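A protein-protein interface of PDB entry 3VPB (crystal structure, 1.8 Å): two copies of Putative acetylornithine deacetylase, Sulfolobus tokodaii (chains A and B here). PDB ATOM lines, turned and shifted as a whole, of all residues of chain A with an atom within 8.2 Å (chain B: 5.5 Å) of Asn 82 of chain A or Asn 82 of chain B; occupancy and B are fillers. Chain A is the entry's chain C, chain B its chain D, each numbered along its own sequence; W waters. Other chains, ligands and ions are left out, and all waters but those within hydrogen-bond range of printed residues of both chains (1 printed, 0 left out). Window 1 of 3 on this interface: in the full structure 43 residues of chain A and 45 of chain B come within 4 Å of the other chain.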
ATOM      1  N   MET A  57     -16.740  33.782  24.647  1.00  0.00           N
ATOM      2  CA  MET A  57     -15.506  33.323  25.325  1.00  0.00           C
ATOM      3  C   MET A  57     -14.304  34.228  25.045  1.00  0.00           C
ATOM      4  O   MET A  57     -13.571  34.586  25.970  1.00  0.00           O
ATOM      5  CB  MET A  57     -15.146  31.867  24.955  1.00  0.00           C
ATOM      6  CG  MET A  57     -14.098  31.215  25.899  1.00  0.00           C
ATOM      7  SD  MET A  57     -12.345  31.573  25.529  1.00  0.00           S
ATOM      8  CE  MET A  57     -11.495  30.250  26.417  1.00  0.00           C
ATOM      9  N   ALA A  60     -14.555  37.510  26.856  1.00  0.00           N
ATOM     10  CA  ALA A  60     -14.266  37.348  28.282  1.00  0.00           C
ATOM     11  C   ALA A  60     -12.762  37.202  28.484  1.00  0.00           C
ATOM     12  O   ALA A  60     -12.185  37.831  29.359  1.00  0.00           O
ATOM     13  CB  ALA A  60     -15.022  36.122  28.877  1.00  0.00           C
ATOM     14  N   LEU A  61     -12.132  36.335  27.695  1.00  0.00           N
ATOM     15  CA  LEU A  61     -10.690  36.102  27.839  1.00  0.00           C
ATOM     16  C   LEU A  61      -9.872  37.369  27.612  1.00  0.00           C
ATOM     17  O   LEU A  61      -9.029  37.746  28.433  1.00  0.00           O
ATOM     18  CB  LEU A  61     -10.237  35.003  26.863  1.00  0.00           C
ATOM     19  CG  LEU A  61      -8.738  34.702  26.835  1.00  0.00           C
ATOM     20  CD1 LEU A  61      -8.300  34.084  28.159  1.00  0.00           C
ATOM     21  CD2 LEU A  61      -8.366  33.783  25.689  1.00  0.00           C
ATOM     22  N   TYR A  62     -10.121  38.043  26.504  1.00  0.00           N
ATOM     23  CA  TYR A  62      -9.316  39.237  26.182  1.00  0.00           C
ATOM     24  C   TYR A  62      -9.618  40.487  27.046  1.00  0.00           C
ATOM     25  O   TYR A  62      -8.685  41.230  27.399  1.00  0.00           O
ATOM     26  CB  TYR A  62      -9.425  39.551  24.695  1.00  0.00           C
ATOM     27  CG  TYR A  62      -8.941  38.444  23.801  1.00  0.00           C
ATOM     28  CD1 TYR A  62      -9.600  38.147  22.602  1.00  0.00           C
ATOM     29  CD2 TYR A  62      -7.810  37.697  24.131  1.00  0.00           C
ATOM     30  CE1 TYR A  62      -9.137  37.139  21.780  1.00  0.00           C
ATOM     31  CE2 TYR A  62      -7.346  36.678  23.315  1.00  0.00           C
ATOM     32  CZ  TYR A  62      -8.012  36.418  22.134  1.00  0.00           C
ATOM     33  OH  TYR A  62      -7.572  35.411  21.327  1.00  0.00           O
ATOM     34  N   SER A  64     -10.518  40.295  30.178  1.00  0.00           N
ATOM     35  CA  SER A  64      -9.819  39.937  31.438  1.00  0.00           C
ATOM     36  C   SER A  64      -8.334  40.254  31.357  1.00  0.00           C
ATOM     37  O   SER A  64      -7.747  40.833  32.290  1.00  0.00           O
ATOM     38  CB  SER A  64      -9.994  38.448  31.754  1.00  0.00           C
ATOM     39  OG  SER A  64      -9.575  38.182  33.077  1.00  0.00           O
ATOM     40  N   ASN A  76     -13.644  36.020  36.474  1.00  0.00           N
ATOM     41  CA  ASN A  76     -12.451  35.198  36.704  1.00  0.00           C
ATOM     42  C   ASN A  76     -11.188  35.719  36.015  1.00  0.00           C
ATOM     43  O   ASN A  76     -11.270  36.580  35.147  1.00  0.00           O
ATOM     44  CB  ASN A  76     -12.719  33.761  36.246  1.00  0.00           C
ATOM     45  CG  ASN A  76     -13.783  33.086  37.073  1.00  0.00           C
ATOM     46  OD1 ASN A  76     -13.603  32.864  38.266  1.00  0.00           O
ATOM     47  ND2 ASN A  76     -14.904  32.770  36.451  1.00  0.00           N
ATOM     48  N   SER A  77     -10.033  35.186  36.409  1.00  0.00           N
ATOM     49  CA  SER A  77      -8.758  35.570  35.792  1.00  0.00           C
ATOM     50  C   SER A  77      -8.628  35.011  34.372  1.00  0.00           C
ATOM     51  O   SER A  77      -9.277  34.009  34.027  1.00  0.00           O
ATOM     52  CB  SER A  77      -7.599  35.067  36.626  1.00  0.00           C
ATOM     53  OG  SER A  77      -7.560  33.647  36.527  1.00  0.00           O
ATOM     54  N   SER A  78      -7.773  35.634  33.557  1.00  0.00           N
ATOM     55  CA  SER A  78      -7.585  35.180  32.176  1.00  0.00           C
ATOM     56  C   SER A  78      -7.079  33.726  32.107  1.00  0.00           C
ATOM     57  O   SER A  78      -7.479  32.971  31.220  1.00  0.00           O
ATOM     58  CB  SER A  78      -6.641  36.114  31.411  1.00  0.00           C
ATOM     59  OG  SER A  78      -5.328  35.980  31.913  1.00  0.00           O
ATOM     60  N   ASP A  79      -6.238  33.304  33.046  1.00  0.00           N
ATOM     61  CA  ASP A  79      -5.797  31.903  32.993  1.00  0.00           C
ATOM     62  C   ASP A  79      -6.903  30.916  33.357  1.00  0.00           C
ATOM     63  O   ASP A  79      -6.967  29.830  32.784  1.00  0.00           O
ATOM     64  CB  ASP A  79      -4.502  31.633  33.770  1.00  0.00           C
ATOM     65  CG  ASP A  79      -4.553  32.093  35.205  1.00  0.00           C
ATOM     66  OD1 ASP A  79      -5.410  32.937  35.557  1.00  0.00           O
ATOM     67  OD2 ASP A  79      -3.696  31.623  35.997  1.00  0.00           O
ATOM     68  N   VAL A  80      -7.779  31.305  34.282  1.00  0.00           N
ATOM     69  CA  VAL A  80      -8.927  30.471  34.639  1.00  0.00           C
ATOM     70  C   VAL A  80      -9.867  30.393  33.426  1.00  0.00           C
ATOM     71  O   VAL A  80     -10.376  29.333  33.094  1.00  0.00           O
ATOM     72  CB  VAL A  80      -9.678  31.038  35.853  1.00  0.00           C
ATOM     73  CG1 VAL A  80     -11.076  30.484  35.972  1.00  0.00           C
ATOM     74  CG2 VAL A  80      -8.845  30.789  37.144  1.00  0.00           C
ATOM     75  N   ILE A  81     -10.091  31.523  32.779  1.00  0.00           N
ATOM     76  CA  ILE A  81     -10.973  31.533  31.600  1.00  0.00           C
ATOM     77  C   ILE A  81     -10.379  30.629  30.507  1.00  0.00           C
ATOM     78  O   ILE A  81     -11.085  29.853  29.867  1.00  0.00           O
ATOM     79  CB  ILE A  81     -11.210  32.972  31.113  1.00  0.00           C
ATOM     80  CG1 ILE A  81     -12.118  33.717  32.095  1.00  0.00           C
ATOM     81  CG2 ILE A  81     -11.806  33.006  29.685  1.00  0.00           C
ATOM     82  CD1 ILE A  81     -12.146  35.202  31.852  1.00  0.00           C
ATOM     83  N   ASN A  82      -9.078  30.730  30.283  1.00  0.00           N
ATOM     84  CA  ASN A  82      -8.447  29.880  29.275  1.00  0.00           C
ATOM     85  C   ASN A  82      -8.602  28.388  29.590  1.00  0.00           C
ATOM     86  O   ASN A  82      -8.976  27.607  28.722  1.00  0.00           O
ATOM     87  CB  ASN A  82      -6.977  30.241  29.109  1.00  0.00           C
ATOM     88  CG  ASN A  82      -6.617  30.566  27.656  1.00  0.00           C
ATOM     89  OD1 ASN A  82      -7.385  30.295  26.719  1.00  0.00           O
ATOM     90  ND2 ASN A  82      -5.451  31.160  27.472  1.00  0.00           N
ATOM     91  N   VAL A  83      -8.350  28.002  30.835  1.00  0.00           N
ATOM     92  CA  VAL A  83      -8.397  26.596  31.205  1.00  0.00           C
ATOM     93  C   VAL A  83      -9.841  26.067  31.263  1.00  0.00           C
ATOM     94  O   VAL A  83     -10.152  25.037  30.660  1.00  0.00           O
ATOM     95  CB  VAL A  83      -7.662  26.313  32.529  1.00  0.00           C
ATOM     96  CG1 VAL A  83      -7.886  24.857  32.963  1.00  0.00           C
ATOM     97  CG2 VAL A  83      -6.190  26.561  32.371  1.00  0.00           C
ATOM     98  N   CYS A  84     -10.720  26.764  31.972  1.00  0.00           N
ATOM     99  CA  CYS A  84     -12.117  26.311  32.063  1.00  0.00           C
ATOM    100  C   CYS A  84     -12.837  26.381  30.723  1.00  0.00           C
ATOM    101  O   CYS A  84     -13.783  25.649  30.509  1.00  0.00           O
ATOM    102  CB  CYS A  84     -12.913  27.093  33.104  1.00  0.00           C
ATOM    103  SG  CYS A  84     -12.250  26.894  34.729  1.00  0.00           S
ATOM    104  N   GLY A  85     -12.400  27.263  29.836  1.00  0.00           N
ATOM    105  CA  GLY A  85     -13.042  27.417  28.524  1.00  0.00           C
ATOM    106  C   GLY A  85     -12.709  26.277  27.575  1.00  0.00           C
ATOM    107  O   GLY A  85     -13.343  26.116  26.519  1.00  0.00           O
ATOM    108  N   ASP A  86     -11.725  25.477  27.953  1.00  0.00           N
ATOM    109  CA  ASP A  86     -11.256  24.407  27.109  1.00  0.00           C
ATOM    110  C   ASP A  86     -11.289  23.055  27.831  1.00  0.00           C
ATOM    111  O   ASP A  86     -10.583  22.852  28.831  1.00  0.00           O
ATOM    112  CB  ASP A  86      -9.854  24.731  26.632  1.00  0.00           C
ATOM    113  CG  ASP A  86      -9.421  23.825  25.522  1.00  0.00           C
ATOM    114  OD1 ASP A  86      -9.300  24.330  24.382  1.00  0.00           O
ATOM    115  OD2 ASP A  86      -9.240  22.606  25.791  1.00  0.00           O
ATOM    116  N   LYS A  87     -12.121  22.139  27.350  1.00  0.00           N
ATOM    117  CA  LYS A  87     -12.286  20.853  28.053  1.00  0.00           C
ATOM    118  C   LYS A  87     -11.012  20.001  28.150  1.00  0.00           C
ATOM    119  O   LYS A  87     -10.762  19.356  29.178  1.00  0.00           O
ATOM    120  CB  LYS A  87     -13.428  20.029  27.467  1.00  0.00           C
ATOM    121  CG  LYS A  87     -14.817  20.596  27.760  1.00  0.00           C
ATOM    122  CD  LYS A  87     -15.875  19.663  27.164  1.00  0.00           C
ATOM    123  CE  LYS A  87     -17.285  20.164  27.447  1.00  0.00           C
ATOM    124  NZ  LYS A  87     -17.572  21.454  26.757  1.00  0.00           N
ATOM    125  N   ILE A  88     -10.191  20.024  27.097  1.00  0.00           N
ATOM    126  CA  ILE A  88      -8.935  19.277  27.116  1.00  0.00           C
ATOM    127  C   ILE A  88      -8.000  19.818  28.210  1.00  0.00           C
ATOM    128  O   ILE A  88      -7.425  19.051  29.001  1.00  0.00           O
ATOM    129  CB  ILE A  88      -8.301  19.268  25.725  1.00  0.00           C
ATOM    130  CG1 ILE A  88      -9.216  18.480  24.764  1.00  0.00           C
ATOM    131  CG2 ILE A  88      -6.883  18.680  25.758  1.00  0.00           C
ATOM    132  CD1 ILE A  88      -8.803  18.573  23.305  1.00  0.00           C
ATOM    133  N   LEU A  89      -7.853  21.143  28.257  1.00  0.00           N
ATOM    134  CA  LEU A  89      -7.008  21.767  29.296  1.00  0.00           C
ATOM    135  C   LEU A  89      -7.527  21.494  30.702  1.00  0.00           C
ATOM    136  O   LEU A  89      -6.724  21.243  31.634  1.00  0.00           O
ATOM    137  CB  LEU A  89      -6.868  23.291  29.068  1.00  0.00           C
ATOM    138  CG  LEU A  89      -6.304  23.716  27.697  1.00  0.00           C
ATOM    139  CD1 LEU A  89      -6.098  25.220  27.613  1.00  0.00           C
ATOM    140  CD2 LEU A  89      -4.990  22.986  27.344  1.00  0.00           C
ATOM    141  N   THR A  90      -8.844  21.599  30.873  1.00  0.00           N
ATOM    142  CA  THR A  90      -9.470  21.249  32.139  1.00  0.00           C
ATOM    143  C   THR A  90      -9.223  19.779  32.516  1.00  0.00           C
ATOM    144  O   THR A  90      -8.781  19.472  33.634  1.00  0.00           O
ATOM    145  CB  THR A  90     -11.001  21.530  32.102  1.00  0.00           C
ATOM    146  OG1 THR A  90     -11.242  22.911  31.815  1.00  0.00           O
ATOM    147  CG2 THR A  90     -11.667  21.146  33.434  1.00  0.00           C
ATOM    148  N   PRO A 129     -13.458  20.522  22.250  1.00  0.00           N
ATOM    149  CA  PRO A 129     -13.017  21.062  23.527  1.00  0.00           C
ATOM    150  C   PRO A 129     -13.661  22.422  23.847  1.00  0.00           C
ATOM    151  O   PRO A 129     -13.584  22.887  24.988  1.00  0.00           O
ATOM    152  CB  PRO A 129     -11.499  21.186  23.334  1.00  0.00           C
ATOM    153  CG  PRO A 129     -11.318  21.392  21.900  1.00  0.00           C
ATOM    154  CD  PRO A 129     -12.343  20.449  21.288  1.00  0.00           C
ATOM    155  N   ILE A 130     -14.288  23.052  22.851  1.00  0.00           N
ATOM    156  CA  ILE A 130     -14.946  24.338  23.094  1.00  0.00           C
ATOM    157  C   ILE A 130     -16.431  24.241  22.759  1.00  0.00           C
ATOM    158  O   ILE A 130     -16.840  23.429  21.930  1.00  0.00           O
ATOM    159  CB  ILE A 130     -14.226  25.549  22.379  1.00  0.00           C
ATOM    160  CG1 ILE A 130     -14.298  25.429  20.855  1.00  0.00           C
ATOM    161  CG2 ILE A 130     -12.765  25.706  22.886  1.00  0.00           C
ATOM    162  CD1 ILE A 130     -13.815  26.694  20.073  1.00  0.00           C
ATOM    163  N   ASP A 253     -16.391  29.191  33.221  1.00  0.00           N
ATOM    164  CA  ASP A 253     -15.735  30.402  33.770  1.00  0.00           C
ATOM    165  C   ASP A 253     -16.587  31.668  33.716  1.00  0.00           C
ATOM    166  O   ASP A 253     -16.214  32.695  34.301  1.00  0.00           O
ATOM    167  CB  ASP A 253     -14.413  30.651  33.034  1.00  0.00           C
ATOM    168  CG  ASP A 253     -14.570  30.589  31.547  1.00  0.00           C
ATOM    169  OD1 ASP A 253     -15.040  31.583  30.952  1.00  0.00           O
ATOM    170  OD2 ASP A 253     -14.233  29.533  30.963  1.00  0.00           O
ATOM    171  N   MET B  57      -1.142  24.941  15.957  1.00  0.00           N
ATOM    172  CA  MET B  57      -1.152  25.407  17.339  1.00  0.00           C
ATOM    173  C   MET B  57      -2.059  24.585  18.263  1.00  0.00           C
ATOM    174  O   MET B  57      -1.679  24.321  19.433  1.00  0.00           O
ATOM    175  CB  MET B  57      -1.484  26.894  17.424  1.00  0.00           C
ATOM    176  CG  MET B  57      -1.101  27.476  18.757  1.00  0.00           C
ATOM    177  SD  MET B  57      -2.476  27.637  19.904  1.00  0.00           S
ATOM    178  CE  MET B  57      -2.766  29.396  19.721  1.00  0.00           C
ATOM    179  N   LEU B  61      -0.861  22.560  21.521  1.00  0.00           N
ATOM    180  CA  LEU B  61      -1.529  22.800  22.801  1.00  0.00           C
ATOM    181  C   LEU B  61      -2.067  21.518  23.416  1.00  0.00           C
ATOM    182  O   LEU B  61      -1.754  21.177  24.562  1.00  0.00           O
ATOM    183  CB  LEU B  61      -2.656  23.834  22.651  1.00  0.00           C
ATOM    184  CG  LEU B  61      -3.447  24.127  23.942  1.00  0.00           C
ATOM    185  CD1 LEU B  61      -2.565  24.784  25.016  1.00  0.00           C
ATOM    186  CD2 LEU B  61      -4.638  25.014  23.685  1.00  0.00           C
ATOM    187  N   SER B  77       5.532  23.901  27.794  1.00  0.00           N
ATOM    188  CA  SER B  77       4.329  23.516  28.558  1.00  0.00           C
ATOM    189  C   SER B  77       3.041  24.042  27.934  1.00  0.00           C
ATOM    190  O   SER B  77       3.075  25.025  27.189  1.00  0.00           O
ATOM    191  CB  SER B  77       4.422  24.046  29.979  1.00  0.00           C
ATOM    192  OG  SER B  77       4.250  25.462  29.933  1.00  0.00           O
ATOM    193  N   SER B  78       1.900  23.425  28.269  1.00  0.00           N
ATOM    194  CA  SER B  78       0.599  23.839  27.713  1.00  0.00           C
ATOM    195  C   SER B  78       0.299  25.294  28.099  1.00  0.00           C
ATOM    196  O   SER B  78      -0.248  26.043  27.310  1.00  0.00           O
ATOM    197  CB  SER B  78      -0.529  22.920  28.218  1.00  0.00           C
ATOM    198  OG  SER B  78      -0.720  23.132  29.614  1.00  0.00           O
ATOM    199  N   ASP B  79       0.724  25.695  29.298  1.00  0.00           N
ATOM    200  CA  ASP B  79       0.467  27.059  29.787  1.00  0.00           C
ATOM    201  C   ASP B  79       1.244  28.072  28.948  1.00  0.00           C
ATOM    202  O   ASP B  79       0.733  29.142  28.605  1.00  0.00           O
ATOM    203  CB  ASP B  79       0.855  27.185  31.274  1.00  0.00           C
ATOM    204  CG  ASP B  79      -0.088  26.405  32.216  1.00  0.00           C
ATOM    205  OD1 ASP B  79       0.301  26.182  33.393  1.00  0.00           O
ATOM    206  OD2 ASP B  79      -1.205  26.006  31.810  1.00  0.00           O
ATOM    207  N   VAL B  80       2.478  27.723  28.600  1.00  0.00           N
ATOM    208  CA  VAL B  80       3.315  28.578  27.767  1.00  0.00           C
ATOM    209  C   VAL B  80       2.758  28.619  26.344  1.00  0.00           C
ATOM    210  O   VAL B  80       2.738  29.669  25.698  1.00  0.00           O
ATOM    211  CB  VAL B  80       4.761  28.050  27.695  1.00  0.00           C
ATOM    212  CG1 VAL B  80       5.494  28.609  26.452  1.00  0.00           C
ATOM    213  CG2 VAL B  80       5.519  28.411  28.984  1.00  0.00           C
ATOM    214  N   ILE B  81       2.339  27.472  25.834  1.00  0.00           N
ATOM    215  CA  ILE B  81       1.826  27.446  24.450  1.00  0.00           C
ATOM    216  C   ILE B  81       0.591  28.369  24.363  1.00  0.00           C
ATOM    217  O   ILE B  81       0.415  29.132  23.395  1.00  0.00           O
ATOM    218  CB  ILE B  81       1.513  26.008  23.989  1.00  0.00           C
ATOM    219  CG1 ILE B  81       2.814  25.225  23.798  1.00  0.00           C
ATOM    220  CG2 ILE B  81       0.708  25.989  22.690  1.00  0.00           C
ATOM    221  CD1 ILE B  81       2.628  23.677  23.777  1.00  0.00           C
ATOM    222  N   ASN B  82      -0.257  28.285  25.382  1.00  0.00           N
ATOM    223  CA  ASN B  82      -1.491  29.066  25.436  1.00  0.00           C
ATOM    224  C   ASN B  82      -1.216  30.570  25.419  1.00  0.00           C
ATOM    225  O   ASN B  82      -1.812  31.312  24.642  1.00  0.00           O
ATOM    226  CB  ASN B  82      -2.322  28.671  26.653  1.00  0.00           C
ATOM    227  CG  ASN B  82      -3.769  28.313  26.286  1.00  0.00           C
ATOM    228  OD1 ASN B  82      -4.190  28.402  25.114  1.00  0.00           O
ATOM    229  ND2 ASN B  82      -4.540  27.939  27.294  1.00  0.00           N
ATOM    230  N   VAL B  83      -0.291  31.006  26.253  1.00  0.00           N
ATOM    231  CA  VAL B  83       0.078  32.417  26.325  1.00  0.00           C
ATOM    232  C   VAL B  83       0.894  32.889  25.105  1.00  0.00           C
ATOM    233  O   VAL B  83       0.556  33.895  24.476  1.00  0.00           O
ATOM    234  CB  VAL B  83       0.859  32.714  27.618  1.00  0.00           C
ATOM    235  CG1 VAL B  83       1.302  34.187  27.639  1.00  0.00           C
ATOM    236  CG2 VAL B  83       0.001  32.414  28.829  1.00  0.00           C
ATOM    237  N   CYS B  84       1.965  32.172  24.766  1.00  0.00           N
ATOM    238  CA  CYS B  84       2.775  32.568  23.602  1.00  0.00           C
ATOM    239  C   CYS B  84       2.018  32.484  22.294  1.00  0.00           C
ATOM    240  O   CYS B  84       2.290  33.244  21.389  1.00  0.00           O
ATOM    241  CB  CYS B  84       4.048  31.753  23.486  1.00  0.00           C
ATOM    242  SG  CYS B  84       5.180  32.127  24.800  1.00  0.00           S
ATOM    243  N   GLY B  85       1.060  31.573  22.201  1.00  0.00           N
ATOM    244  CA  GLY B  85       0.266  31.445  20.977  1.00  0.00           C
ATOM    245  C   GLY B  85      -0.723  32.587  20.772  1.00  0.00           C
ATOM    246  O   GLY B  85      -1.286  32.748  19.703  1.00  0.00           O
ATOM    247  N   ASP B  86      -0.933  33.382  21.804  1.00  0.00           N
ATOM    248  CA  ASP B  86      -1.933  34.419  21.760  1.00  0.00           C
ATOM    249  C   ASP B  86      -1.314  35.783  22.048  1.00  0.00           C
ATOM    250  O   ASP B  86      -0.806  36.036  23.148  1.00  0.00           O
ATOM    251  CB  ASP B  86      -3.045  34.101  22.750  1.00  0.00           C
ATOM    252  CG  ASP B  86      -4.249  34.992  22.560  1.00  0.00           C
ATOM    253  OD1 ASP B  86      -5.342  34.458  22.268  1.00  0.00           O
ATOM    254  OD2 ASP B  86      -4.101  36.228  22.686  1.00  0.00           O
ATOM    255  N   LEU B  89      -2.756  37.729  25.151  1.00  0.00           N
ATOM    256  CA  LEU B  89      -2.293  37.156  26.422  1.00  0.00           C
ATOM    257  C   LEU B  89      -0.822  37.472  26.681  1.00  0.00           C
ATOM    258  O   LEU B  89      -0.440  37.767  27.829  1.00  0.00           O
ATOM    259  CB  LEU B  89      -2.528  35.626  26.471  1.00  0.00           C
ATOM    260  CG  LEU B  89      -3.994  35.176  26.334  1.00  0.00           C
ATOM    261  CD1 LEU B  89      -4.155  33.710  26.586  1.00  0.00           C
ATOM    262  CD2 LEU B  89      -4.941  35.989  27.231  1.00  0.00           C
HETATM  263  O   HOH W   1      -7.737  27.620  26.043  1.00  0.00           O
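The side-chain carboxylate (OD1) of Asp 86 of chain B sits at hydrogen-bond distance from the side-chain hydroxyl (OH) of Tyr 62 of chain A, at 2.6 Å. The side-chain amide nitrogen (ND2) of Asn 82 of chain A sits close to the side-chain amide nitrogen (ND2) of Asn 82 of chain B, at 3.4 Å.
OD2 of Asp 86 of chain A lies within hydrogen-bond range of N of Leu 89 of chain A (3.2 Å). The side-chain carboxylate (OD2) of Asp 86 of chain B sits at hydrogen-bond distance from the backbone NH (N) of Leu 89 of chain B, at 3.2 Å.
Among the printed residues, pairs that only touch across the chains: Leu 61 of chain A with Leu 89 of chain B, Asn 82 of chain A with Leu 89 of chain B, Leu 89 of chain A with Leu 61 of chain B and Leu 89 of chain A with Asn 82 of chain B.
Asn 82 of chain A touches two residues of chain B. Asn 82 of chain B touches just these residues of chain A: Asn 82 (3.4 Å) and Leu 89 (3.1 Å). Printed residues of chain A within 4 Å of Leu 61 of chain B: Leu 89. Of the printed residues of chain A, Asp 86 of chain B touches Tyr 62. Printed residues of chain A within 4 Å of Leu 89 of chain B: Leu 61 (3.97 Å) and Asn 82 (3.0 Å). The nearest residue of chain B that does not touch Asn 82 of chain A is Val 83 of chain B (5.3 Å). The nearest residue of chain A that does not touch Asn 82 of chain B is Val 83 of chain A (5.2 Å).
Of the 23 printed residues of chain A, 4 touch a printed residue of chain B. Hydrophobic or aromatic side chains of chain A that line the printed part of chain B: Leu 61, Tyr 62 and Leu 89. Of the 13 printed residues of chain B, 4 touch a printed residue of chain A. Hydrophobic or aromatic side chains of chain B within 4 Å of the printed part of chain A: Leu 61 and Leu 89.
Leu 61 of chain A touches Leu 89 of chain B, and with the chains exchanged Leu 89 of chain A touches Leu 61 of chain B. Asn 82 of chain A touches its own counterpart, Asn 82 of chain B. Asn 82 of chain A touches Leu 89 of chain B, and with the chains exchanged Leu 89 of chain A touches Asn 82 of chain B. Positions printed for both chains: 57, 61, 77, 78, 79, 80, 81, 82, 83, 84, 85, 86 and 89. Of the 6 pairs that touch across the chains among the printed residues, 5 have their exchanged pair printed and touching as well.
Water W1 lies within hydrogen-bond range of the side-chain amide oxygen of Asn 82 of chain A and the side-chain amide nitrogen of Asn 82 of chain B.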
